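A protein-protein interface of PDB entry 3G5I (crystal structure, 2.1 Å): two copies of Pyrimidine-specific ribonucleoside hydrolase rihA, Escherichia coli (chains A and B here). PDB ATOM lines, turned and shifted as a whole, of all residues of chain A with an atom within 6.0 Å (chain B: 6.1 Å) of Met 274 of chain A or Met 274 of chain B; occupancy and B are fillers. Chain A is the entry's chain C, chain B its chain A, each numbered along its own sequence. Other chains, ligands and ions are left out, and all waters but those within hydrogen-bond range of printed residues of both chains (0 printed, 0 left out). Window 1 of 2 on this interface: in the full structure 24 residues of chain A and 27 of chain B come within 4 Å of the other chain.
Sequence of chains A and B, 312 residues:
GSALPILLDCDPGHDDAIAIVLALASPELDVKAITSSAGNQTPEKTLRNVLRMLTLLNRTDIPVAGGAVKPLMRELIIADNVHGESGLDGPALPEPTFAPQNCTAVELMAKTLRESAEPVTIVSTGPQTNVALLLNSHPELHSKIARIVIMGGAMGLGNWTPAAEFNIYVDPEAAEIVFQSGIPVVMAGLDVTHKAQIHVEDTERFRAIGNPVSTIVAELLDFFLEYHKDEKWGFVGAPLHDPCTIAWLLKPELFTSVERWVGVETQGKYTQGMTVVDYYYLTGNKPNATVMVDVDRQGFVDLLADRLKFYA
Among the printed residues, pairs that only touch across the chains: Tyr 270 of chain A with Val 264 of chain B, Val 264 of chain A with Tyr 270 of chain B, Val 276 of chain A with Pro 162 of chain B, Pro 162 of chain A with Val 276 of chain B, Val 276 of chain A with Thr 271 of chain B, Thr 271 of chain A with Val 276 of chain B, Met 274 of chain A with Thr 271 of chain B, Thr 271 of chain A with Met 274 of chain B, Val 277 of chain A with Pro 162 of chain B, Pro 162 of chain A with Val 277 of chain B, Gly 263 of chain A with Tyr 270 of chain B, Tyr 270 of chain A with Gly 263 of chain B, Tyr 270 of chain A with Val 276 of chain B and Val 276 of chain A with Tyr 270 of chain B.
Pro 162 of chain A touches Val 276 of chain B, and with the chains exchanged Val 276 of chain A touches Pro 162 of chain B.
Pro 162 of chain A touches Val 277 of chain B, and with the chains exchanged Val 277 of chain A touches Pro 162 of chain B.
Val 264 of chain A touches Tyr 270 of chain B, and with the chains exchanged Tyr 270 of chain A touches Val 264 of chain B.
Met 274 of chain B touches its own counterpart, Met 274 of chain A.
Hydrophobic or aromatic side chains of chain A that line the printed part of chain B: Pro 162, Tyr 270, Met 274 and Val 276.
Hydrophobic or aromatic side chains of chain B within 4 Å of the printed part of chain A: Pro 162, Tyr 270, Met 274 and Val 276.
Among the printed residues, no Asp or Glu carboxylate lies within 4 Å of a Lys or Arg side-chain nitrogen of the other chain.
Glu 165 of chain A touches none of the printed residues of chain B.
Printed residues of chain B within 4 Å of Gly 263 of chain A: Tyr 270.
Of chain B, only Thr 271 and Met 274 come within 4 Å of Met 274 of chain A.
Of the printed residues of chain A, Tyr 270 of chain B touches Gly 263 (3.7 Å), Val 264 (3.3 Å), Glu 265 (2.6 Å) and Val 276 (3.8 Å).
Met 274 of chain B touches just these residues of chain A: Thr 271 (3.7 Å) and Met 274 (3.5 Å).
Printed residues of chain A within 4 Å of Val 277 of chain B: Pro 162 (3.7 Å).
The nearest residue of chain A that does not touch Met 274 of chain B is Ala 163 of chain A (4.2 Å).
The side-chain carboxylate (OE1) of Glu 265 of chain B lies within hydrogen-bond range of the backbone NH (N) of Tyr 270 of chain A, 2.6 Å away.
The backbone NH (N) of Tyr 270 of chain B sits at hydrogen-bond distance from the side-chain carboxylate (OE1) of Glu 265 of chain A (2.6 Å).
The side-chain carboxylate (OE1) of Glu 265 of chain B lies within hydrogen-bond range of the side-chain hydroxyl (OG1) of Thr 271 of chain A, 3.2 Å away.
The side-chain hydroxyl of Thr 271 of chain B sits at hydrogen-bond distance from the side-chain carboxylate of Glu 265 of chain A (2.9 Å).
The side-chain hydroxyl (OG1) of Thr 271 of chain A is in hydrogen-bond range of the side-chain hydroxyl (OG1) of Thr 271 of chain B (2.8 Å).
SD of Met 274 of chain A sits close to SD of Met 274 of chain B, at 3.5 Å.
O of Glu 265 of chain B lies within hydrogen-bond range of N of Gly 273 of chain B (2.8 Å).
N of Gly 273 of chain A sits at hydrogen-bond distance from O of Glu 265 of chain A (2.8 Å).
N of Val 276 of chain B lies within hydrogen-bond range of O of Gly 263 of chain B, at 2.7 Å.
N of Glu 265 of chain A is in hydrogen-bond range of O of Met 274 of chain A (2.9 Å).
O of Gly 263 of chain A lies within hydrogen-bond range of N of Val 276 of chain A (2.8 Å).
The backbone carbonyl oxygen (O) of Met 274 of chain B sits at hydrogen-bond distance from the backbone NH (N) of Glu 265 of chain B (2.9 Å).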
ATOM      1  N   ALA A 154     -23.712  25.861  22.496  1.00  0.00           N
ATOM      2  CA  ALA A 154     -23.092  26.951  23.245  1.00  0.00           C
ATOM      3  C   ALA A 154     -21.656  26.507  23.480  1.00  0.00           C
ATOM      4  O   ALA A 154     -21.438  25.393  23.948  1.00  0.00           O
ATOM      5  CB  ALA A 154     -23.807  27.155  24.616  1.00  0.00           C
ATOM      6  N   MET A 155     -20.683  27.343  23.134  1.00  0.00           N
ATOM      7  CA  MET A 155     -19.297  27.077  23.497  1.00  0.00           C
ATOM      8  C   MET A 155     -19.168  27.255  25.010  1.00  0.00           C
ATOM      9  O   MET A 155     -18.497  26.462  25.714  1.00  0.00           O
ATOM     10  CB  MET A 155     -18.370  28.010  22.715  1.00  0.00           C
ATOM     11  CG  MET A 155     -16.917  27.981  23.127  1.00  0.00           C
ATOM     12  SD  MET A 155     -15.852  28.570  21.800  1.00  0.00           S
ATOM     13  CE  MET A 155     -16.284  30.334  21.735  1.00  0.00           C
ATOM     14  N   GLY A 156     -19.832  28.280  25.526  1.00  0.00           N
ATOM     15  CA  GLY A 156     -19.917  28.501  26.966  1.00  0.00           C
ATOM     16  C   GLY A 156     -21.119  27.841  27.578  1.00  0.00           C
ATOM     17  O   GLY A 156     -21.537  26.796  27.121  1.00  0.00           O
ATOM     18  N   PRO A 162     -26.742  22.956  32.689  1.00  0.00           N
ATOM     19  CA  PRO A 162     -25.494  23.741  32.795  1.00  0.00           C
ATOM     20  C   PRO A 162     -24.610  23.689  31.548  1.00  0.00           C
ATOM     21  O   PRO A 162     -24.058  24.720  31.134  1.00  0.00           O
ATOM     22  CB  PRO A 162     -24.799  23.093  34.009  1.00  0.00           C
ATOM     23  CG  PRO A 162     -25.927  22.709  34.870  1.00  0.00           C
ATOM     24  CD  PRO A 162     -26.964  22.164  33.926  1.00  0.00           C
ATOM     25  N   ALA A 163     -24.546  22.526  30.903  1.00  0.00           N
ATOM     26  CA  ALA A 163     -23.597  22.316  29.820  1.00  0.00           C
ATOM     27  C   ALA A 163     -24.257  22.429  28.455  1.00  0.00           C
ATOM     28  O   ALA A 163     -23.604  22.604  27.461  1.00  0.00           O
ATOM     29  CB  ALA A 163     -22.945  20.983  30.009  1.00  0.00           C
ATOM     30  N   ALA A 164     -25.573  22.413  28.408  1.00  0.00           N
ATOM     31  CA  ALA A 164     -26.205  22.231  27.102  1.00  0.00           C
ATOM     32  C   ALA A 164     -27.296  23.244  26.703  1.00  0.00           C
ATOM     33  O   ALA A 164     -28.132  23.644  27.535  1.00  0.00           O
ATOM     34  CB  ALA A 164     -26.785  20.853  27.053  1.00  0.00           C
ATOM     35  N   GLU A 165     -27.300  23.617  25.427  1.00  0.00           N
ATOM     36  CA  GLU A 165     -28.353  24.456  24.868  1.00  0.00           C
ATOM     37  C   GLU A 165     -29.531  23.547  24.464  1.00  0.00           C
ATOM     38  O   GLU A 165     -29.353  22.367  24.131  1.00  0.00           O
ATOM     39  CB  GLU A 165     -27.797  25.272  23.683  1.00  0.00           C
ATOM     40  CG  GLU A 165     -28.800  26.127  22.969  1.00  0.00           C
ATOM     41  CD  GLU A 165     -29.547  25.354  21.878  1.00  0.00           C
ATOM     42  OE1 GLU A 165     -29.008  24.376  21.356  1.00  0.00           O
ATOM     43  OE2 GLU A 165     -30.678  25.729  21.560  1.00  0.00           O
ATOM     44  N   ILE A 168     -29.935  21.280  20.993  1.00  0.00           N
ATOM     45  CA  ILE A 168     -28.988  20.176  20.951  1.00  0.00           C
ATOM     46  C   ILE A 168     -29.373  19.114  22.015  1.00  0.00           C
ATOM     47  O   ILE A 168     -29.409  17.901  21.741  1.00  0.00           O
ATOM     48  CB  ILE A 168     -27.530  20.630  21.176  1.00  0.00           C
ATOM     49  CG1 ILE A 168     -27.132  21.739  20.186  1.00  0.00           C
ATOM     50  CG2 ILE A 168     -26.587  19.379  21.033  1.00  0.00           C
ATOM     51  CD1 ILE A 168     -27.234  21.379  18.608  1.00  0.00           C
ATOM     52  N   GLY A 263     -17.692  18.653  18.785  1.00  0.00           N
ATOM     53  CA  GLY A 263     -18.281  17.303  19.000  1.00  0.00           C
ATOM     54  C   GLY A 263     -19.506  17.424  19.900  1.00  0.00           C
ATOM     55  O   GLY A 263     -19.479  18.254  20.746  1.00  0.00           O
ATOM     56  N   VAL A 264     -20.550  16.606  19.763  1.00  0.00           N
ATOM     57  CA  VAL A 264     -21.739  16.707  20.658  1.00  0.00           C
ATOM     58  C   VAL A 264     -21.747  15.534  21.587  1.00  0.00           C
ATOM     59  O   VAL A 264     -21.632  14.386  21.159  1.00  0.00           O
ATOM     60  CB  VAL A 264     -23.025  16.714  19.830  1.00  0.00           C
ATOM     61  CG1 VAL A 264     -24.256  16.625  20.712  1.00  0.00           C
ATOM     62  CG2 VAL A 264     -23.094  17.986  18.920  1.00  0.00           C
ATOM     63  N   GLU A 265     -21.819  15.812  22.892  1.00  0.00           N
ATOM     64  CA  GLU A 265     -21.741  14.801  23.916  1.00  0.00           C
ATOM     65  C   GLU A 265     -23.073  14.063  23.898  1.00  0.00           C
ATOM     66  O   GLU A 265     -24.142  14.699  24.006  1.00  0.00           O
ATOM     67  CB  GLU A 265     -21.519  15.459  25.283  1.00  0.00           C
ATOM     68  CG  GLU A 265     -21.362  14.419  26.409  1.00  0.00           C
ATOM     69  CD  GLU A 265     -20.241  13.447  26.106  1.00  0.00           C
ATOM     70  OE1 GLU A 265     -19.091  13.911  26.001  1.00  0.00           O
ATOM     71  OE2 GLU A 265     -20.518  12.250  25.944  1.00  0.00           O
ATOM     72  N   TYR A 270     -23.373  14.276  33.076  1.00  0.00           N
ATOM     73  CA  TYR A 270     -23.791  15.651  33.385  1.00  0.00           C
ATOM     74  C   TYR A 270     -23.796  16.534  32.148  1.00  0.00           C
ATOM     75  O   TYR A 270     -24.121  17.724  32.230  1.00  0.00           O
ATOM     76  CB  TYR A 270     -22.772  16.251  34.364  1.00  0.00           C
ATOM     77  CG  TYR A 270     -22.762  15.663  35.758  1.00  0.00           C
ATOM     78  CD1 TYR A 270     -23.954  15.468  36.461  1.00  0.00           C
ATOM     79  CD2 TYR A 270     -21.549  15.323  36.373  1.00  0.00           C
ATOM     80  CE1 TYR A 270     -23.945  14.931  37.759  1.00  0.00           C
ATOM     81  CE2 TYR A 270     -21.512  14.804  37.620  1.00  0.00           C
ATOM     82  CZ  TYR A 270     -22.710  14.610  38.326  1.00  0.00           C
ATOM     83  OH  TYR A 270     -22.636  14.115  39.566  1.00  0.00           O
ATOM     84  N   THR A 271     -23.370  15.983  31.015  1.00  0.00           N
ATOM     85  CA  THR A 271     -23.052  16.777  29.881  1.00  0.00           C
ATOM     86  C   THR A 271     -23.724  16.320  28.612  1.00  0.00           C
ATOM     87  O   THR A 271     -23.282  16.687  27.549  1.00  0.00           O
ATOM     88  CB  THR A 271     -21.521  16.751  29.617  1.00  0.00           C
ATOM     89  OG1 THR A 271     -21.069  15.372  29.581  1.00  0.00           O
ATOM     90  CG2 THR A 271     -20.803  17.529  30.731  1.00  0.00           C
ATOM     91  N   GLN A 272     -24.790  15.521  28.698  1.00  0.00           N
ATOM     92  CA  GLN A 272     -25.527  15.188  27.436  1.00  0.00           C
ATOM     93  C   GLN A 272     -26.000  16.442  26.713  1.00  0.00           C
ATOM     94  O   GLN A 272     -26.515  17.330  27.348  1.00  0.00           O
ATOM     95  CB  GLN A 272     -26.637  14.133  27.650  1.00  0.00           C
ATOM     96  CG  GLN A 272     -25.990  12.709  27.825  1.00  0.00           C
ATOM     97  CD  GLN A 272     -26.995  11.629  28.286  1.00  0.00           C
ATOM     98  OE1 GLN A 272     -27.948  11.279  27.556  1.00  0.00           O
ATOM     99  NE2 GLN A 272     -26.749  11.044  29.462  1.00  0.00           N
ATOM    100  N   GLY A 273     -25.745  16.533  25.408  1.00  0.00           N
ATOM    101  CA  GLY A 273     -26.153  17.716  24.628  1.00  0.00           C
ATOM    102  C   GLY A 273     -25.175  18.861  24.529  1.00  0.00           C
ATOM    103  O   GLY A 273     -25.417  19.846  23.833  1.00  0.00           O
ATOM    104  N   MET A 274     -24.038  18.758  25.219  1.00  0.00           N
ATOM    105  CA  MET A 274     -23.036  19.820  25.161  1.00  0.00           C
ATOM    106  C   MET A 274     -22.385  19.793  23.798  1.00  0.00           C
ATOM    107  O   MET A 274     -22.050  18.671  23.298  1.00  0.00           O
ATOM    108  CB  MET A 274     -21.922  19.558  26.176  1.00  0.00           C
ATOM    109  CG  MET A 274     -20.929  20.691  26.163  1.00  0.00           C
ATOM    110  SD  MET A 274     -19.787  20.425  27.438  1.00  0.00           S
ATOM    111  CE  MET A 274     -18.658  21.784  27.241  1.00  0.00           C
ATOM    112  N   THR A 275     -22.265  20.972  23.180  1.00  0.00           N
ATOM    113  CA  THR A 275     -21.377  21.137  22.016  1.00  0.00           C
ATOM    114  C   THR A 275     -19.955  21.478  22.521  1.00  0.00           C
ATOM    115  O   THR A 275     -19.698  22.578  23.014  1.00  0.00           O
ATOM    116  CB  THR A 275     -21.924  22.270  21.051  1.00  0.00           C
ATOM    117  OG1 THR A 275     -22.078  23.523  21.755  1.00  0.00           O
ATOM    118  CG2 THR A 275     -23.263  21.878  20.525  1.00  0.00           C
ATOM    119  N   VAL A 276     -19.029  20.525  22.358  1.00  0.00           N
ATOM    120  CA  VAL A 276     -17.667  20.679  22.794  1.00  0.00           C
ATOM    121  C   VAL A 276     -16.919  21.312  21.624  1.00  0.00           C
ATOM    122  O   VAL A 276     -16.656  20.638  20.577  1.00  0.00           O
ATOM    123  CB  VAL A 276     -17.130  19.263  23.243  1.00  0.00           C
ATOM    124  CG1 VAL A 276     -15.617  19.292  23.601  1.00  0.00           C
ATOM    125  CG2 VAL A 276     -17.937  18.794  24.475  1.00  0.00           C
ATOM    126  N   VAL A 277     -16.534  22.583  21.799  1.00  0.00           N
ATOM    127  CA  VAL A 277     -15.862  23.325  20.744  1.00  0.00           C
ATOM    128  C   VAL A 277     -14.410  23.388  21.061  1.00  0.00           C
ATOM    129  O   VAL A 277     -14.062  23.883  22.123  1.00  0.00           O
ATOM    130  CB  VAL A 277     -16.437  24.751  20.547  1.00  0.00           C
ATOM    131  CG1 VAL A 277     -15.780  25.399  19.302  1.00  0.00           C
ATOM    132  CG2 VAL A 277     -17.943  24.699  20.320  1.00  0.00           C
ATOM    133  N   ALA B 154     -12.948  24.439  35.442  1.00  0.00           N
ATOM    134  CA  ALA B 154     -13.179  25.655  34.708  1.00  0.00           C
ATOM    135  C   ALA B 154     -14.643  25.689  34.417  1.00  0.00           C
ATOM    136  O   ALA B 154     -15.190  24.720  33.959  1.00  0.00           O
ATOM    137  CB  ALA B 154     -12.412  25.649  33.431  1.00  0.00           C
ATOM    138  N   MET B 155     -15.289  26.804  34.687  1.00  0.00           N
ATOM    139  CA  MET B 155     -16.696  26.926  34.327  1.00  0.00           C
ATOM    140  C   MET B 155     -16.779  27.110  32.796  1.00  0.00           C
ATOM    141  O   MET B 155     -17.703  26.609  32.139  1.00  0.00           O
ATOM    142  CB  MET B 155     -17.322  28.073  35.117  1.00  0.00           C
ATOM    143  CG  MET B 155     -18.711  28.439  34.732  1.00  0.00           C
ATOM    144  SD  MET B 155     -19.323  29.396  36.121  1.00  0.00           S
ATOM    145  CE  MET B 155     -18.523  30.963  35.908  1.00  0.00           C
ATOM    146  N   GLY B 156     -15.791  27.779  32.208  1.00  0.00           N
ATOM    147  CA  GLY B 156     -15.762  27.914  30.756  1.00  0.00           C
ATOM    148  C   GLY B 156     -14.758  26.925  30.220  1.00  0.00           C
ATOM    149  O   GLY B 156     -14.658  25.809  30.757  1.00  0.00           O
ATOM    150  N   PRO B 162     -10.825  20.437  25.331  1.00  0.00           N
ATOM    151  CA  PRO B 162     -11.800  21.527  25.180  1.00  0.00           C
ATOM    152  C   PRO B 162     -12.632  21.867  26.434  1.00  0.00           C
ATOM    153  O   PRO B 162     -12.832  23.044  26.727  1.00  0.00           O
ATOM    154  CB  PRO B 162     -12.682  21.021  24.028  1.00  0.00           C
ATOM    155  CG  PRO B 162     -11.681  20.360  23.174  1.00  0.00           C
ATOM    156  CD  PRO B 162     -10.789  19.601  24.119  1.00  0.00           C
ATOM    157  N   ALA B 163     -12.983  20.849  27.203  1.00  0.00           N
ATOM    158  CA  ALA B 163     -13.961  20.987  28.277  1.00  0.00           C
ATOM    159  C   ALA B 163     -13.331  20.830  29.647  1.00  0.00           C
ATOM    160  O   ALA B 163     -13.929  21.169  30.673  1.00  0.00           O
ATOM    161  CB  ALA B 163     -15.038  19.944  28.060  1.00  0.00           C
ATOM    162  N   ALA B 164     -12.089  20.382  29.701  1.00  0.00           N
ATOM    163  CA  ALA B 164     -11.524  20.084  31.006  1.00  0.00           C
ATOM    164  C   ALA B 164     -10.221  20.723  31.344  1.00  0.00           C
ATOM    165  O   ALA B 164      -9.316  20.834  30.511  1.00  0.00           O
ATOM    166  CB  ALA B 164     -11.428  18.531  31.202  1.00  0.00           C
ATOM    167  N   GLU B 165     -10.094  21.083  32.611  1.00  0.00           N
ATOM    168  CA  GLU B 165      -8.850  21.611  33.146  1.00  0.00           C
ATOM    169  C   GLU B 165      -7.997  20.430  33.614  1.00  0.00           C
ATOM    170  O   GLU B 165      -8.508  19.400  33.981  1.00  0.00           O
ATOM    171  CB  GLU B 165      -9.149  22.651  34.261  1.00  0.00           C
ATOM    172  CG  GLU B 165      -7.913  23.261  34.998  1.00  0.00           C
ATOM    173  CD  GLU B 165      -7.348  22.331  36.075  1.00  0.00           C
ATOM    174  OE1 GLU B 165      -8.118  21.577  36.697  1.00  0.00           O
ATOM    175  OE2 GLU B 165      -6.137  22.365  36.312  1.00  0.00           O
ATOM    176  N   ILE B 168      -8.270  18.332  37.148  1.00  0.00           N
ATOM    177  CA  ILE B 168      -9.521  17.562  37.195  1.00  0.00           C
ATOM    178  C   ILE B 168      -9.467  16.436  36.185  1.00  0.00           C
ATOM    179  O   ILE B 168      -9.860  15.313  36.494  1.00  0.00           O
ATOM    180  CB  ILE B 168     -10.781  18.427  36.982  1.00  0.00           C
ATOM    181  CG1 ILE B 168     -10.887  19.573  38.007  1.00  0.00           C
ATOM    182  CG2 ILE B 168     -12.032  17.560  37.138  1.00  0.00           C
ATOM    183  CD1 ILE B 168     -10.837  19.255  39.584  1.00  0.00           C
ATOM    184  N   GLY B 263     -20.717  19.593  39.346  1.00  0.00           N
ATOM    185  CA  GLY B 263     -20.572  18.159  39.115  1.00  0.00           C
ATOM    186  C   GLY B 263     -19.315  17.871  38.304  1.00  0.00           C
ATOM    187  O   GLY B 263     -18.926  18.684  37.461  1.00  0.00           O
ATOM    188  N   VAL B 264     -18.653  16.737  38.525  1.00  0.00           N
ATOM    189  CA  VAL B 264     -17.516  16.437  37.663  1.00  0.00           C
ATOM    190  C   VAL B 264     -17.881  15.263  36.741  1.00  0.00           C
ATOM    191  O   VAL B 264     -18.412  14.266  37.225  1.00  0.00           O
ATOM    192  CB  VAL B 264     -16.287  16.112  38.459  1.00  0.00           C
ATOM    193  CG1 VAL B 264     -15.091  15.625  37.488  1.00  0.00           C
ATOM    194  CG2 VAL B 264     -15.894  17.313  39.331  1.00  0.00           C
ATOM    195  N   GLU B 265     -17.637  15.426  35.427  1.00  0.00           N
ATOM    196  CA  GLU B 265     -18.025  14.458  34.399  1.00  0.00           C
ATOM    197  C   GLU B 265     -16.978  13.335  34.419  1.00  0.00           C
ATOM    198  O   GLU B 265     -15.737  13.594  34.349  1.00  0.00           O
ATOM    199  CB  GLU B 265     -18.090  15.091  33.009  1.00  0.00           C
ATOM    200  CG  GLU B 265     -18.518  14.141  31.940  1.00  0.00           C
ATOM    201  CD  GLU B 265     -19.870  13.499  32.247  1.00  0.00           C
ATOM    202  OE1 GLU B 265     -20.845  14.251  32.527  1.00  0.00           O
ATOM    203  OE2 GLU B 265     -19.966  12.245  32.221  1.00  0.00           O
ATOM    204  N   THR B 266     -17.463  12.109  34.540  1.00  0.00           N
ATOM    205  CA  THR B 266     -16.531  10.998  34.610  1.00  0.00           C
ATOM    206  C   THR B 266     -16.734   9.993  33.447  1.00  0.00           C
ATOM    207  O   THR B 266     -15.878   9.079  33.232  1.00  0.00           O
ATOM    208  CB  THR B 266     -16.556  10.290  35.944  1.00  0.00           C
ATOM    209  OG1 THR B 266     -17.833   9.759  36.144  1.00  0.00           O
ATOM    210  CG2 THR B 266     -16.274  11.260  37.148  1.00  0.00           C
ATOM    211  N   TYR B 270     -16.711  13.182  25.229  1.00  0.00           N
ATOM    212  CA  TYR B 270     -15.912  14.342  24.857  1.00  0.00           C
ATOM    213  C   TYR B 270     -15.583  15.190  26.066  1.00  0.00           C
ATOM    214  O   TYR B 270     -14.833  16.138  25.949  1.00  0.00           O
ATOM    215  CB  TYR B 270     -16.699  15.206  23.833  1.00  0.00           C
ATOM    216  CG  TYR B 270     -16.918  14.559  22.513  1.00  0.00           C
ATOM    217  CD1 TYR B 270     -15.864  14.042  21.792  1.00  0.00           C
ATOM    218  CD2 TYR B 270     -18.173  14.508  21.945  1.00  0.00           C
ATOM    219  CE1 TYR B 270     -16.064  13.457  20.535  1.00  0.00           C
ATOM    220  CE2 TYR B 270     -18.378  13.946  20.712  1.00  0.00           C
ATOM    221  CZ  TYR B 270     -17.311  13.423  20.000  1.00  0.00           C
ATOM    222  OH  TYR B 270     -17.509  12.853  18.758  1.00  0.00           O
ATOM    223  N   THR B 271     -16.132  14.848  27.227  1.00  0.00           N
ATOM    224  CA  THR B 271     -16.174  15.787  28.333  1.00  0.00           C
ATOM    225  C   THR B 271     -15.632  15.242  29.668  1.00  0.00           C
ATOM    226  O   THR B 271     -15.964  15.787  30.725  1.00  0.00           O
ATOM    227  CB  THR B 271     -17.678  16.178  28.617  1.00  0.00           C
ATOM    228  OG1 THR B 271     -18.451  14.986  28.616  1.00  0.00           O
ATOM    229  CG2 THR B 271     -18.260  17.115  27.531  1.00  0.00           C
ATOM    230  N   GLN B 272     -14.823  14.182  29.638  1.00  0.00           N
ATOM    231  CA  GLN B 272     -14.297  13.628  30.875  1.00  0.00           C
ATOM    232  C   GLN B 272     -13.434  14.689  31.570  1.00  0.00           C
ATOM    233  O   GLN B 272     -12.597  15.333  30.931  1.00  0.00           O
ATOM    234  CB  GLN B 272     -13.603  12.265  30.670  1.00  0.00           C
ATOM    235  CG  GLN B 272     -14.640  11.094  30.589  1.00  0.00           C
ATOM    236  CD  GLN B 272     -14.018   9.724  30.255  1.00  0.00           C
ATOM    237  OE1 GLN B 272     -13.337   9.109  31.091  1.00  0.00           O
ATOM    238  NE2 GLN B 272     -14.271   9.220  29.017  1.00  0.00           N
ATOM    239  N   GLY B 273     -13.737  14.941  32.837  1.00  0.00           N
ATOM    240  CA  GLY B 273     -13.002  15.920  33.607  1.00  0.00           C
ATOM    241  C   GLY B 273     -13.567  17.329  33.608  1.00  0.00           C
ATOM    242  O   GLY B 273     -13.019  18.204  34.270  1.00  0.00           O
ATOM    243  N   MET B 274     -14.667  17.554  32.884  1.00  0.00           N
ATOM    244  CA  MET B 274     -15.348  18.805  32.954  1.00  0.00           C
ATOM    245  C   MET B 274     -15.879  18.999  34.319  1.00  0.00           C
ATOM    246  O   MET B 274     -16.467  18.071  34.896  1.00  0.00           O
ATOM    247  CB  MET B 274     -16.532  18.840  31.987  1.00  0.00           C
ATOM    248  CG  MET B 274     -17.114  20.219  31.847  1.00  0.00           C
ATOM    249  SD  MET B 274     -18.304  20.218  30.568  1.00  0.00           S
ATOM    250  CE  MET B 274     -18.937  21.907  30.749  1.00  0.00           C
ATOM    251  N   THR B 275     -15.706  20.217  34.833  1.00  0.00           N
ATOM    252  CA  THR B 275     -16.490  20.667  35.969  1.00  0.00           C
ATOM    253  C   THR B 275     -17.710  21.381  35.468  1.00  0.00           C
ATOM    254  O   THR B 275     -17.583  22.440  34.858  1.00  0.00           O
ATOM    255  CB  THR B 275     -15.721  21.661  36.859  1.00  0.00           C
ATOM    256  OG1 THR B 275     -15.318  22.776  36.052  1.00  0.00           O
ATOM    257  CG2 THR B 275     -14.541  20.980  37.554  1.00  0.00           C
ATOM    258  N   VAL B 276     -18.887  20.814  35.771  1.00  0.00           N
ATOM    259  CA  VAL B 276     -20.149  21.305  35.302  1.00  0.00           C
ATOM    260  C   VAL B 276     -20.690  22.183  36.462  1.00  0.00           C
ATOM    261  O   VAL B 276     -20.990  21.670  37.551  1.00  0.00           O
ATOM    262  CB  VAL B 276     -21.100  20.111  34.917  1.00  0.00           C
ATOM    263  CG1 VAL B 276     -22.416  20.578  34.454  1.00  0.00           C
ATOM    264  CG2 VAL B 276     -20.460  19.227  33.861  1.00  0.00           C
ATOM    265  N   VAL B 277     -20.772  23.499  36.229  1.00  0.00           N
ATOM    266  CA  VAL B 277     -21.145  24.413  37.261  1.00  0.00           C
ATOM    267  C   VAL B 277     -22.515  24.949  36.914  1.00  0.00           C
ATOM    268  O   VAL B 277     -22.690  25.563  35.823  1.00  0.00           O
ATOM    269  CB  VAL B 277     -20.138  25.591  37.424  1.00  0.00           C
ATOM    270  CG1 VAL B 277     -20.583  26.476  38.625  1.00  0.00           C
ATOM    271  CG2 VAL B 277     -18.659  25.125  37.650  1.00  0.00           C
